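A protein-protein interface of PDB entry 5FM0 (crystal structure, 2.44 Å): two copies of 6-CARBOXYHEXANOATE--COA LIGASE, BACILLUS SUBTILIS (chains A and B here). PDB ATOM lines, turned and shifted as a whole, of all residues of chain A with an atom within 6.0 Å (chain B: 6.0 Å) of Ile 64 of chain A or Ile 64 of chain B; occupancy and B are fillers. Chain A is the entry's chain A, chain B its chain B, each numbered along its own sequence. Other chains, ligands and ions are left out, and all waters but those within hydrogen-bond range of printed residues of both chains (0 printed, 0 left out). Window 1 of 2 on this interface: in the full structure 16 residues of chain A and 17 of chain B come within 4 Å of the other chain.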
ATOM      1  N   VAL A  11     -26.914  16.009 -13.271  1.00  0.00           N
ATOM      2  CA  VAL A  11     -26.018  15.385 -12.309  1.00  0.00           C
ATOM      3  C   VAL A  11     -24.591  15.604 -12.758  1.00  0.00           C
ATOM      4  O   VAL A  11     -24.243  15.255 -13.870  1.00  0.00           O
ATOM      5  CB  VAL A  11     -26.284  13.875 -12.169  1.00  0.00           C
ATOM      6  CG1 VAL A  11     -25.553  13.315 -10.955  1.00  0.00           C
ATOM      7  CG2 VAL A  11     -27.761  13.627 -12.014  1.00  0.00           C
ATOM      8  N   ARG A  12     -23.772  16.170 -11.883  1.00  0.00           N
ATOM      9  CA  ARG A  12     -22.395  16.547 -12.226  1.00  0.00           C
ATOM     10  C   ARG A  12     -21.388  16.009 -11.220  1.00  0.00           C
ATOM     11  O   ARG A  12     -21.687  15.846 -10.044  1.00  0.00           O
ATOM     12  CB  ARG A  12     -22.238  18.061 -12.250  1.00  0.00           C
ATOM     13  CG  ARG A  12     -22.967  18.750 -13.383  1.00  0.00           C
ATOM     14  CD  ARG A  12     -22.832  20.285 -13.297  1.00  0.00           C
ATOM     15  NE  ARG A  12     -23.816  20.866 -12.394  1.00  0.00           N
ATOM     16  CZ  ARG A  12     -23.687  22.037 -11.773  1.00  0.00           C
ATOM     17  NH1 ARG A  12     -22.608  22.791 -11.943  1.00  0.00           N
ATOM     18  NH2 ARG A  12     -24.660  22.456 -10.980  1.00  0.00           N
ATOM     19  N   MET A  13     -20.175  15.779 -11.693  1.00  0.00           N
ATOM     20  CA  MET A  13     -19.112  15.270 -10.859  1.00  0.00           C
ATOM     21  C   MET A  13     -17.810  15.945 -11.235  1.00  0.00           C
ATOM     22  O   MET A  13     -17.557  16.215 -12.405  1.00  0.00           O
ATOM     23  CB  MET A  13     -18.989  13.762 -11.048  1.00  0.00           C
ATOM     24  CG  MET A  13     -17.902  13.107 -10.212  1.00  0.00           C
ATOM     25  SD  MET A  13     -16.272  13.259 -10.967  1.00  0.00           S
ATOM     26  CE  MET A  13     -16.433  12.160 -12.380  1.00  0.00           C
ATOM     27  N   ARG A  14     -16.981  16.229 -10.240  1.00  0.00           N
ATOM     28  CA  ARG A  14     -15.578  16.562 -10.494  1.00  0.00           C
ATOM     29  C   ARG A  14     -14.666  15.944  -9.428  1.00  0.00           C
ATOM     30  O   ARG A  14     -15.072  15.732  -8.290  1.00  0.00           O
ATOM     31  CB  ARG A  14     -15.364  18.062 -10.617  1.00  0.00           C
ATOM     32  CG  ARG A  14     -15.734  18.890  -9.406  1.00  0.00           C
ATOM     33  CD  ARG A  14     -15.417  20.360  -9.678  1.00  0.00           C
ATOM     34  NE  ARG A  14     -15.197  21.136  -8.455  1.00  0.00           N
ATOM     35  CZ  ARG A  14     -16.116  21.911  -7.887  1.00  0.00           C
ATOM     36  NH1 ARG A  14     -17.334  22.032  -8.425  1.00  0.00           N
ATOM     37  NH2 ARG A  14     -15.817  22.567  -6.776  1.00  0.00           N
ATOM     38  N   VAL A  44     -25.455   8.313 -10.022  1.00  0.00           N
ATOM     39  CA  VAL A  44     -24.525   8.760  -8.988  1.00  0.00           C
ATOM     40  C   VAL A  44     -23.417   7.739  -8.837  1.00  0.00           C
ATOM     41  O   VAL A  44     -22.235   8.088  -8.769  1.00  0.00           O
ATOM     42  CB  VAL A  44     -25.217   9.013  -7.638  1.00  0.00           C
ATOM     43  CG1 VAL A  44     -24.185   9.189  -6.546  1.00  0.00           C
ATOM     44  CG2 VAL A  44     -26.080  10.250  -7.738  1.00  0.00           C
ATOM     45  N   LEU A  47     -21.020   7.847 -11.938  1.00  0.00           N
ATOM     46  CA  LEU A  47     -20.103   8.968 -11.873  1.00  0.00           C
ATOM     47  C   LEU A  47     -19.052   8.745 -10.811  1.00  0.00           C
ATOM     48  O   LEU A  47     -17.893   9.136 -10.971  1.00  0.00           O
ATOM     49  CB  LEU A  47     -20.855  10.265 -11.583  1.00  0.00           C
ATOM     50  CG  LEU A  47     -21.671  10.778 -12.752  1.00  0.00           C
ATOM     51  CD1 LEU A  47     -22.654  11.836 -12.266  1.00  0.00           C
ATOM     52  CD2 LEU A  47     -20.772  11.317 -13.854  1.00  0.00           C
ATOM     53  N   LEU A  48     -19.473   8.166  -9.699  1.00  0.00           N
ATOM     54  CA  LEU A  48     -18.547   7.835  -8.637  1.00  0.00           C
ATOM     55  C   LEU A  48     -17.464   6.900  -9.181  1.00  0.00           C
ATOM     56  O   LEU A  48     -16.278   7.168  -9.072  1.00  0.00           O
ATOM     57  CB  LEU A  48     -19.299   7.153  -7.509  1.00  0.00           C
ATOM     58  CG  LEU A  48     -18.446   6.772  -6.313  1.00  0.00           C
ATOM     59  CD1 LEU A  48     -17.621   7.954  -5.799  1.00  0.00           C
ATOM     60  CD2 LEU A  48     -19.355   6.219  -5.239  1.00  0.00           C
ATOM     61  N   MET A  62     -13.584  14.851  -4.363  1.00  0.00           N
ATOM     62  CA  MET A  62     -14.637  14.639  -5.316  1.00  0.00           C
ATOM     63  C   MET A  62     -15.939  15.318  -4.887  1.00  0.00           C
ATOM     64  O   MET A  62     -16.274  15.338  -3.716  1.00  0.00           O
ATOM     65  CB  MET A  62     -14.886  13.156  -5.526  1.00  0.00           C
ATOM     66  CG  MET A  62     -15.923  12.889  -6.618  1.00  0.00           C
ATOM     67  SD  MET A  62     -16.244  11.149  -6.990  1.00  0.00           S
ATOM     68  CE  MET A  62     -14.609  10.585  -7.409  1.00  0.00           C
ATOM     69  N   GLN A  63     -16.654  15.874  -5.867  1.00  0.00           N
ATOM     70  CA  GLN A  63     -17.967  16.449  -5.679  1.00  0.00           C
ATOM     71  C   GLN A  63     -18.918  15.823  -6.662  1.00  0.00           C
ATOM     72  O   GLN A  63     -18.661  15.809  -7.840  1.00  0.00           O
ATOM     73  CB  GLN A  63     -17.968  17.932  -5.955  1.00  0.00           C
ATOM     74  CG  GLN A  63     -17.566  18.826  -4.814  1.00  0.00           C
ATOM     75  CD  GLN A  63     -18.265  20.179  -4.877  1.00  0.00           C
ATOM     76  OE1 GLN A  63     -19.394  20.291  -5.376  1.00  0.00           O
ATOM     77  NE2 GLN A  63     -17.594  21.215  -4.376  1.00  0.00           N
ATOM     78  N   ILE A  64     -20.036  15.351  -6.160  1.00  0.00           N
ATOM     79  CA  ILE A  64     -21.104  14.946  -6.970  1.00  0.00           C
ATOM     80  C   ILE A  64     -22.315  15.730  -6.549  1.00  0.00           C
ATOM     81  O   ILE A  64     -22.599  15.887  -5.364  1.00  0.00           O
ATOM     82  CB  ILE A  64     -21.432  13.482  -6.784  1.00  0.00           C
ATOM     83  CG1 ILE A  64     -20.256  12.630  -7.246  1.00  0.00           C
ATOM     84  CG2 ILE A  64     -22.709  13.144  -7.550  1.00  0.00           C
ATOM     85  CD1 ILE A  64     -20.418  11.170  -6.925  1.00  0.00           C
ATOM     86  N   GLN A  65     -23.066  16.186  -7.531  1.00  0.00           N
ATOM     87  CA  GLN A  65     -24.158  17.079  -7.266  1.00  0.00           C
ATOM     88  C   GLN A  65     -25.316  16.875  -8.259  1.00  0.00           C
ATOM     89  O   GLN A  65     -25.103  16.520  -9.422  1.00  0.00           O
ATOM     90  CB  GLN A  65     -23.624  18.504  -7.331  1.00  0.00           C
ATOM     91  CG  GLN A  65     -24.658  19.507  -7.753  1.00  0.00           C
ATOM     92  CD  GLN A  65     -24.146  20.917  -7.669  1.00  0.00           C
ATOM     93  OE1 GLN A  65     -23.084  21.169  -7.124  1.00  0.00           O
ATOM     94  NE2 GLN A  65     -24.916  21.847  -8.200  1.00  0.00           N
ATOM     95  N   PHE A  66     -26.540  17.070  -7.798  1.00  0.00           N
ATOM     96  CA  PHE A  66     -27.660  17.079  -8.716  1.00  0.00           C
ATOM     97  C   PHE A  66     -28.636  18.208  -8.437  1.00  0.00           C
ATOM     98  O   PHE A  66     -28.646  18.783  -7.346  1.00  0.00           O
ATOM     99  CB  PHE A  66     -28.346  15.729  -8.779  1.00  0.00           C
ATOM    100  CG  PHE A  66     -29.207  15.403  -7.605  1.00  0.00           C
ATOM    101  CD1 PHE A  66     -30.392  16.075  -7.388  1.00  0.00           C
ATOM    102  CD2 PHE A  66     -28.879  14.354  -6.763  1.00  0.00           C
ATOM    103  CE1 PHE A  66     -31.215  15.738  -6.325  1.00  0.00           C
ATOM    104  CE2 PHE A  66     -29.693  14.003  -5.697  1.00  0.00           C
ATOM    105  CZ  PHE A  66     -30.868  14.700  -5.477  1.00  0.00           C
ATOM    106  N   VAL B  11     -16.530  12.734   4.303  1.00  0.00           N
ATOM    107  CA  VAL B  11     -17.599  12.657   3.315  1.00  0.00           C
ATOM    108  C   VAL B  11     -18.806  13.413   3.856  1.00  0.00           C
ATOM    109  O   VAL B  11     -19.276  13.132   4.967  1.00  0.00           O
ATOM    110  CB  VAL B  11     -18.005  11.202   2.999  1.00  0.00           C
ATOM    111  CG1 VAL B  11     -18.897  11.149   1.768  1.00  0.00           C
ATOM    112  CG2 VAL B  11     -16.776  10.343   2.764  1.00  0.00           C
ATOM    113  N   ARG B  12     -19.296  14.377   3.080  1.00  0.00           N
ATOM    114  CA  ARG B  12     -20.396  15.274   3.520  1.00  0.00           C
ATOM    115  C   ARG B  12     -21.497  15.324   2.505  1.00  0.00           C
ATOM    116  O   ARG B  12     -21.263  15.200   1.305  1.00  0.00           O
ATOM    117  CB  ARG B  12     -19.882  16.692   3.736  1.00  0.00           C
ATOM    118  CG  ARG B  12     -18.954  16.822   4.933  1.00  0.00           C
ATOM    119  CD  ARG B  12     -18.518  18.246   5.140  1.00  0.00           C
ATOM    120  NE  ARG B  12     -17.956  18.795   3.918  1.00  0.00           N
ATOM    121  CZ  ARG B  12     -17.890  20.091   3.643  1.00  0.00           C
ATOM    122  NH1 ARG B  12     -18.338  20.992   4.505  1.00  0.00           N
ATOM    123  NH2 ARG B  12     -17.371  20.482   2.499  1.00  0.00           N
ATOM    124  N   MET B  13     -22.699  15.551   2.989  1.00  0.00           N
ATOM    125  CA  MET B  13     -23.857  15.658   2.135  1.00  0.00           C
ATOM    126  C   MET B  13     -24.788  16.766   2.609  1.00  0.00           C
ATOM    127  O   MET B  13     -24.951  16.978   3.820  1.00  0.00           O
ATOM    128  CB  MET B  13     -24.618  14.334   2.144  1.00  0.00           C
ATOM    129  CG  MET B  13     -25.867  14.303   1.263  1.00  0.00           C
ATOM    130  SD  MET B  13     -27.318  15.001   2.052  1.00  0.00           S
ATOM    131  CE  MET B  13     -27.663  13.813   3.357  1.00  0.00           C
ATOM    132  N   ARG B  14     -25.402  17.473   1.657  1.00  0.00           N
ATOM    133  CA  ARG B  14     -26.545  18.337   1.981  1.00  0.00           C
ATOM    134  C   ARG B  14     -27.602  18.279   0.894  1.00  0.00           C
ATOM    135  O   ARG B  14     -27.297  18.086  -0.268  1.00  0.00           O
ATOM    136  CB  ARG B  14     -26.109  19.767   2.276  1.00  0.00           C
ATOM    137  CG  ARG B  14     -25.352  20.452   1.160  1.00  0.00           C
ATOM    138  CD  ARG B  14     -24.965  21.852   1.609  1.00  0.00           C
ATOM    139  NE  ARG B  14     -24.787  22.775   0.493  1.00  0.00           N
ATOM    140  CZ  ARG B  14     -23.611  23.132  -0.011  1.00  0.00           C
ATOM    141  NH1 ARG B  14     -22.476  22.637   0.488  1.00  0.00           N
ATOM    142  NH2 ARG B  14     -23.569  23.989  -1.021  1.00  0.00           N
ATOM    143  N   VAL B  44     -21.062   6.806   0.358  1.00  0.00           N
ATOM    144  CA  VAL B  44     -21.705   7.706  -0.585  1.00  0.00           C
ATOM    145  C   VAL B  44     -23.141   7.280  -0.781  1.00  0.00           C
ATOM    146  O   VAL B  44     -24.053   8.127  -0.761  1.00  0.00           O
ATOM    147  CB  VAL B  44     -20.962   7.790  -1.906  1.00  0.00           C
ATOM    148  CG1 VAL B  44     -21.797   8.522  -2.944  1.00  0.00           C
ATOM    149  CG2 VAL B  44     -19.656   8.524  -1.695  1.00  0.00           C
ATOM    150  N   LEU B  47     -25.314   8.054   2.351  1.00  0.00           N
ATOM    151  CA  LEU B  47     -25.656   9.468   2.411  1.00  0.00           C
ATOM    152  C   LEU B  47     -26.691   9.825   1.371  1.00  0.00           C
ATOM    153  O   LEU B  47     -27.607  10.617   1.630  1.00  0.00           O
ATOM    154  CB  LEU B  47     -24.435  10.350   2.228  1.00  0.00           C
ATOM    155  CG  LEU B  47     -23.489  10.321   3.410  1.00  0.00           C
ATOM    156  CD1 LEU B  47     -22.148  10.914   2.992  1.00  0.00           C
ATOM    157  CD2 LEU B  47     -24.087  11.070   4.601  1.00  0.00           C
ATOM    158  N   LEU B  48     -26.536   9.248   0.193  1.00  0.00           N
ATOM    159  CA  LEU B  48     -27.495   9.448  -0.864  1.00  0.00           C
ATOM    160  C   LEU B  48     -28.859   9.027  -0.403  1.00  0.00           C
ATOM    161  O   LEU B  48     -29.806   9.806  -0.457  1.00  0.00           O
ATOM    162  CB  LEU B  48     -27.096   8.638  -2.068  1.00  0.00           C
ATOM    163  CG  LEU B  48     -28.011   8.790  -3.263  1.00  0.00           C
ATOM    164  CD1 LEU B  48     -28.249  10.253  -3.622  1.00  0.00           C
ATOM    165  CD2 LEU B  48     -27.384   8.036  -4.437  1.00  0.00           C
ATOM    166  N   MET B  62     -28.937  18.351  -4.228  1.00  0.00           N
ATOM    167  CA  MET B  62     -28.105  17.603  -3.326  1.00  0.00           C
ATOM    168  C   MET B  62     -26.670  17.726  -3.746  1.00  0.00           C
ATOM    169  O   MET B  62     -26.367  17.777  -4.942  1.00  0.00           O
ATOM    170  CB  MET B  62     -28.501  16.125  -3.298  1.00  0.00           C
ATOM    171  CG  MET B  62     -27.689  15.325  -2.279  1.00  0.00           C
ATOM    172  SD  MET B  62     -28.104  13.573  -2.070  1.00  0.00           S
ATOM    173  CE  MET B  62     -29.849  13.693  -1.719  1.00  0.00           C
ATOM    174  N   GLN B  63     -25.790  17.787  -2.750  1.00  0.00           N
ATOM    175  CA  GLN B  63     -24.357  17.783  -2.951  1.00  0.00           C
ATOM    176  C   GLN B  63     -23.759  16.721  -2.088  1.00  0.00           C
ATOM    177  O   GLN B  63     -24.011  16.682  -0.878  1.00  0.00           O
ATOM    178  CB  GLN B  63     -23.734  19.086  -2.489  1.00  0.00           C
ATOM    179  CG  GLN B  63     -23.707  20.196  -3.495  1.00  0.00           C
ATOM    180  CD  GLN B  63     -22.500  21.094  -3.303  1.00  0.00           C
ATOM    181  OE1 GLN B  63     -21.444  20.646  -2.836  1.00  0.00           O
ATOM    182  NE2 GLN B  63     -22.638  22.359  -3.677  1.00  0.00           N
ATOM    183  N   ILE B  64     -22.917  15.891  -2.677  1.00  0.00           N
ATOM    184  CA  ILE B  64     -22.122  14.970  -1.902  1.00  0.00           C
ATOM    185  C   ILE B  64     -20.693  15.192  -2.232  1.00  0.00           C
ATOM    186  O   ILE B  64     -20.334  15.317  -3.391  1.00  0.00           O
ATOM    187  CB  ILE B  64     -22.448  13.515  -2.237  1.00  0.00           C
ATOM    188  CG1 ILE B  64     -23.878  13.200  -1.810  1.00  0.00           C
ATOM    189  CG2 ILE B  64     -21.464  12.597  -1.538  1.00  0.00           C
ATOM    190  CD1 ILE B  64     -24.357  11.842  -2.281  1.00  0.00           C
ATOM    191  N   GLN B  65     -19.854  15.184  -1.215  1.00  0.00           N
ATOM    192  CA  GLN B  65     -18.473  15.521  -1.409  1.00  0.00           C
ATOM    193  C   GLN B  65     -17.550  14.718  -0.481  1.00  0.00           C
ATOM    194  O   GLN B  65     -17.929  14.371   0.614  1.00  0.00           O
ATOM    195  CB  GLN B  65     -18.319  17.001  -1.170  1.00  0.00           C
ATOM    196  CG  GLN B  65     -16.978  17.383  -0.637  1.00  0.00           C
ATOM    197  CD  GLN B  65     -16.844  18.869  -0.468  1.00  0.00           C
ATOM    198  OE1 GLN B  65     -17.533  19.644  -1.133  1.00  0.00           O
ATOM    199  NE2 GLN B  65     -15.936  19.280   0.411  1.00  0.00           N
ATOM    200  N   PHE B  66     -16.343  14.409  -0.942  1.00  0.00           N
ATOM    201  CA  PHE B  66     -15.347  13.824  -0.076  1.00  0.00           C
ATOM    202  C   PHE B  66     -14.023  14.440  -0.296  1.00  0.00           C
ATOM    203  O   PHE B  66     -13.746  15.006  -1.356  1.00  0.00           O
ATOM    204  CB  PHE B  66     -15.287  12.290  -0.193  1.00  0.00           C
ATOM    205  CG  PHE B  66     -14.600  11.759  -1.424  1.00  0.00           C
ATOM    206  CD1 PHE B  66     -13.224  11.820  -1.565  1.00  0.00           C
ATOM    207  CD2 PHE B  66     -15.325  11.099  -2.392  1.00  0.00           C
ATOM    208  CE1 PHE B  66     -12.598  11.275  -2.681  1.00  0.00           C
ATOM    209  CE2 PHE B  66     -14.706  10.550  -3.504  1.00  0.00           C
ATOM    210  CZ  PHE B  66     -13.338  10.638  -3.650  1.00  0.00           C
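Val 44 of chain A touches Leu 48 of chain B, but with the chains exchanged Leu 48 of chain A does not touch Val 44 of chain B (4.02 Å). Met 62 of chain A touches Gln 65 of chain B, and with the chains exchanged Gln 65 of chain A touches Met 62 of chain B. Met 62 of chain A touches Phe 66 of chain B, and with the chains exchanged Phe 66 of chain A touches Met 62 of chain B. Gln 63 of chain A touches Ile 64 of chain B, and with the chains exchanged Ile 64 of chain A touches Gln 63 of chain B. 12 positions are printed for both chains.
The backbone carbonyl oxygen (O) of Met 62 of chain B lies within hydrogen-bond range of the backbone NH (N) of Phe 66 of chain A, 2.9 Å away. The side-chain amide oxygen (OE1) of Gln 63 of chain A sits close to the side-chain amide oxygen (OE1) of Gln 63 of chain B (3.3 Å). O of Ile 64 of chain A lies within hydrogen-bond range of N of Ile 64 of chain B. The backbone carbonyl oxygen (O) of Met 62 of chain A is in hydrogen-bond range of the backbone NH (N) of Phe 66 of chain B, 2.9 Å away.
Printed residues of chain B that touch a printed residue of chain A: Leu 48, Met 62, Gln 63, Ile 64, Gln 65 and Phe 66. Along chain B the printed residues that touch a printed residue of chain A span positions 48 to 66. Hydrophobic or aromatic side chains of chain A that line the printed part of chain B: Val 44, Met 62 and Phe 66. Among the printed residues, no Asp or Glu carboxylate lies within 4 Å of a Lys or Arg side-chain nitrogen of the other chain.
The backbone NH (N) of Arg 12 of chain A is in hydrogen-bond range of the backbone carbonyl oxygen (O) of Gln 65 of chain A. The guanidinium group (NH2) of Arg 12 of chain B lies close to the side-chain amide nitrogen (NE2) of Gln 65 of chain B, at 2.8 Å. The backbone NH of Gln 63 of chain A is in hydrogen-bond range of the backbone carbonyl oxygen of Arg 14 of chain A (2.9 Å). N of Gln 63 of chain B is in hydrogen-bond range of O of Arg 14 of chain B (2.9 Å).
Among the printed residues, pairs that only touch across the chains: Val 44 of chain A with Leu 48 of chain B, Met 62 of chain A with Gln 65 of chain B, Gln 63 of chain A with Ile 64 of chain B, Gln 63 of chain A with Gln 65 of chain B, Ile 64 of chain A with Gln 63 of chain B, Gln 65 of chain A with Met 62 of chain B and Gln 65 of chain A with Gln 63 of chain B.
Met 13 of chain A touches none of the printed residues of chain B. Printed residues of chain B within 4 Å of Gln 63 of chain A: Gln 63, Ile 64 and Gln 65. Of chain B, only Gln 63 (3.5 Å) and Ile 64 (2.7 Å) come within 4 Å of Ile 64 of chain A. Printed residues of chain B within 4 Å of Gln 65 of chain A: Met 62 and Gln 63. Arg 14 of chain B touches none of the printed residues of chain A. Printed residues of chain A within 4 Å of Ile 64 of chain B: Gln 63 and Ile 64. Of the printed residues of chain A, Gln 65 of chain B touches Met 62 (3.2 Å) and Gln 63 (3.6 Å). The nearest residue of chain B that does not touch Ile 64 of chain A is Met 62 of chain B (4.2 Å). The nearest residue of chain A that does not touch Ile 64 of chain B is Met 62 of chain A (4.1 Å).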
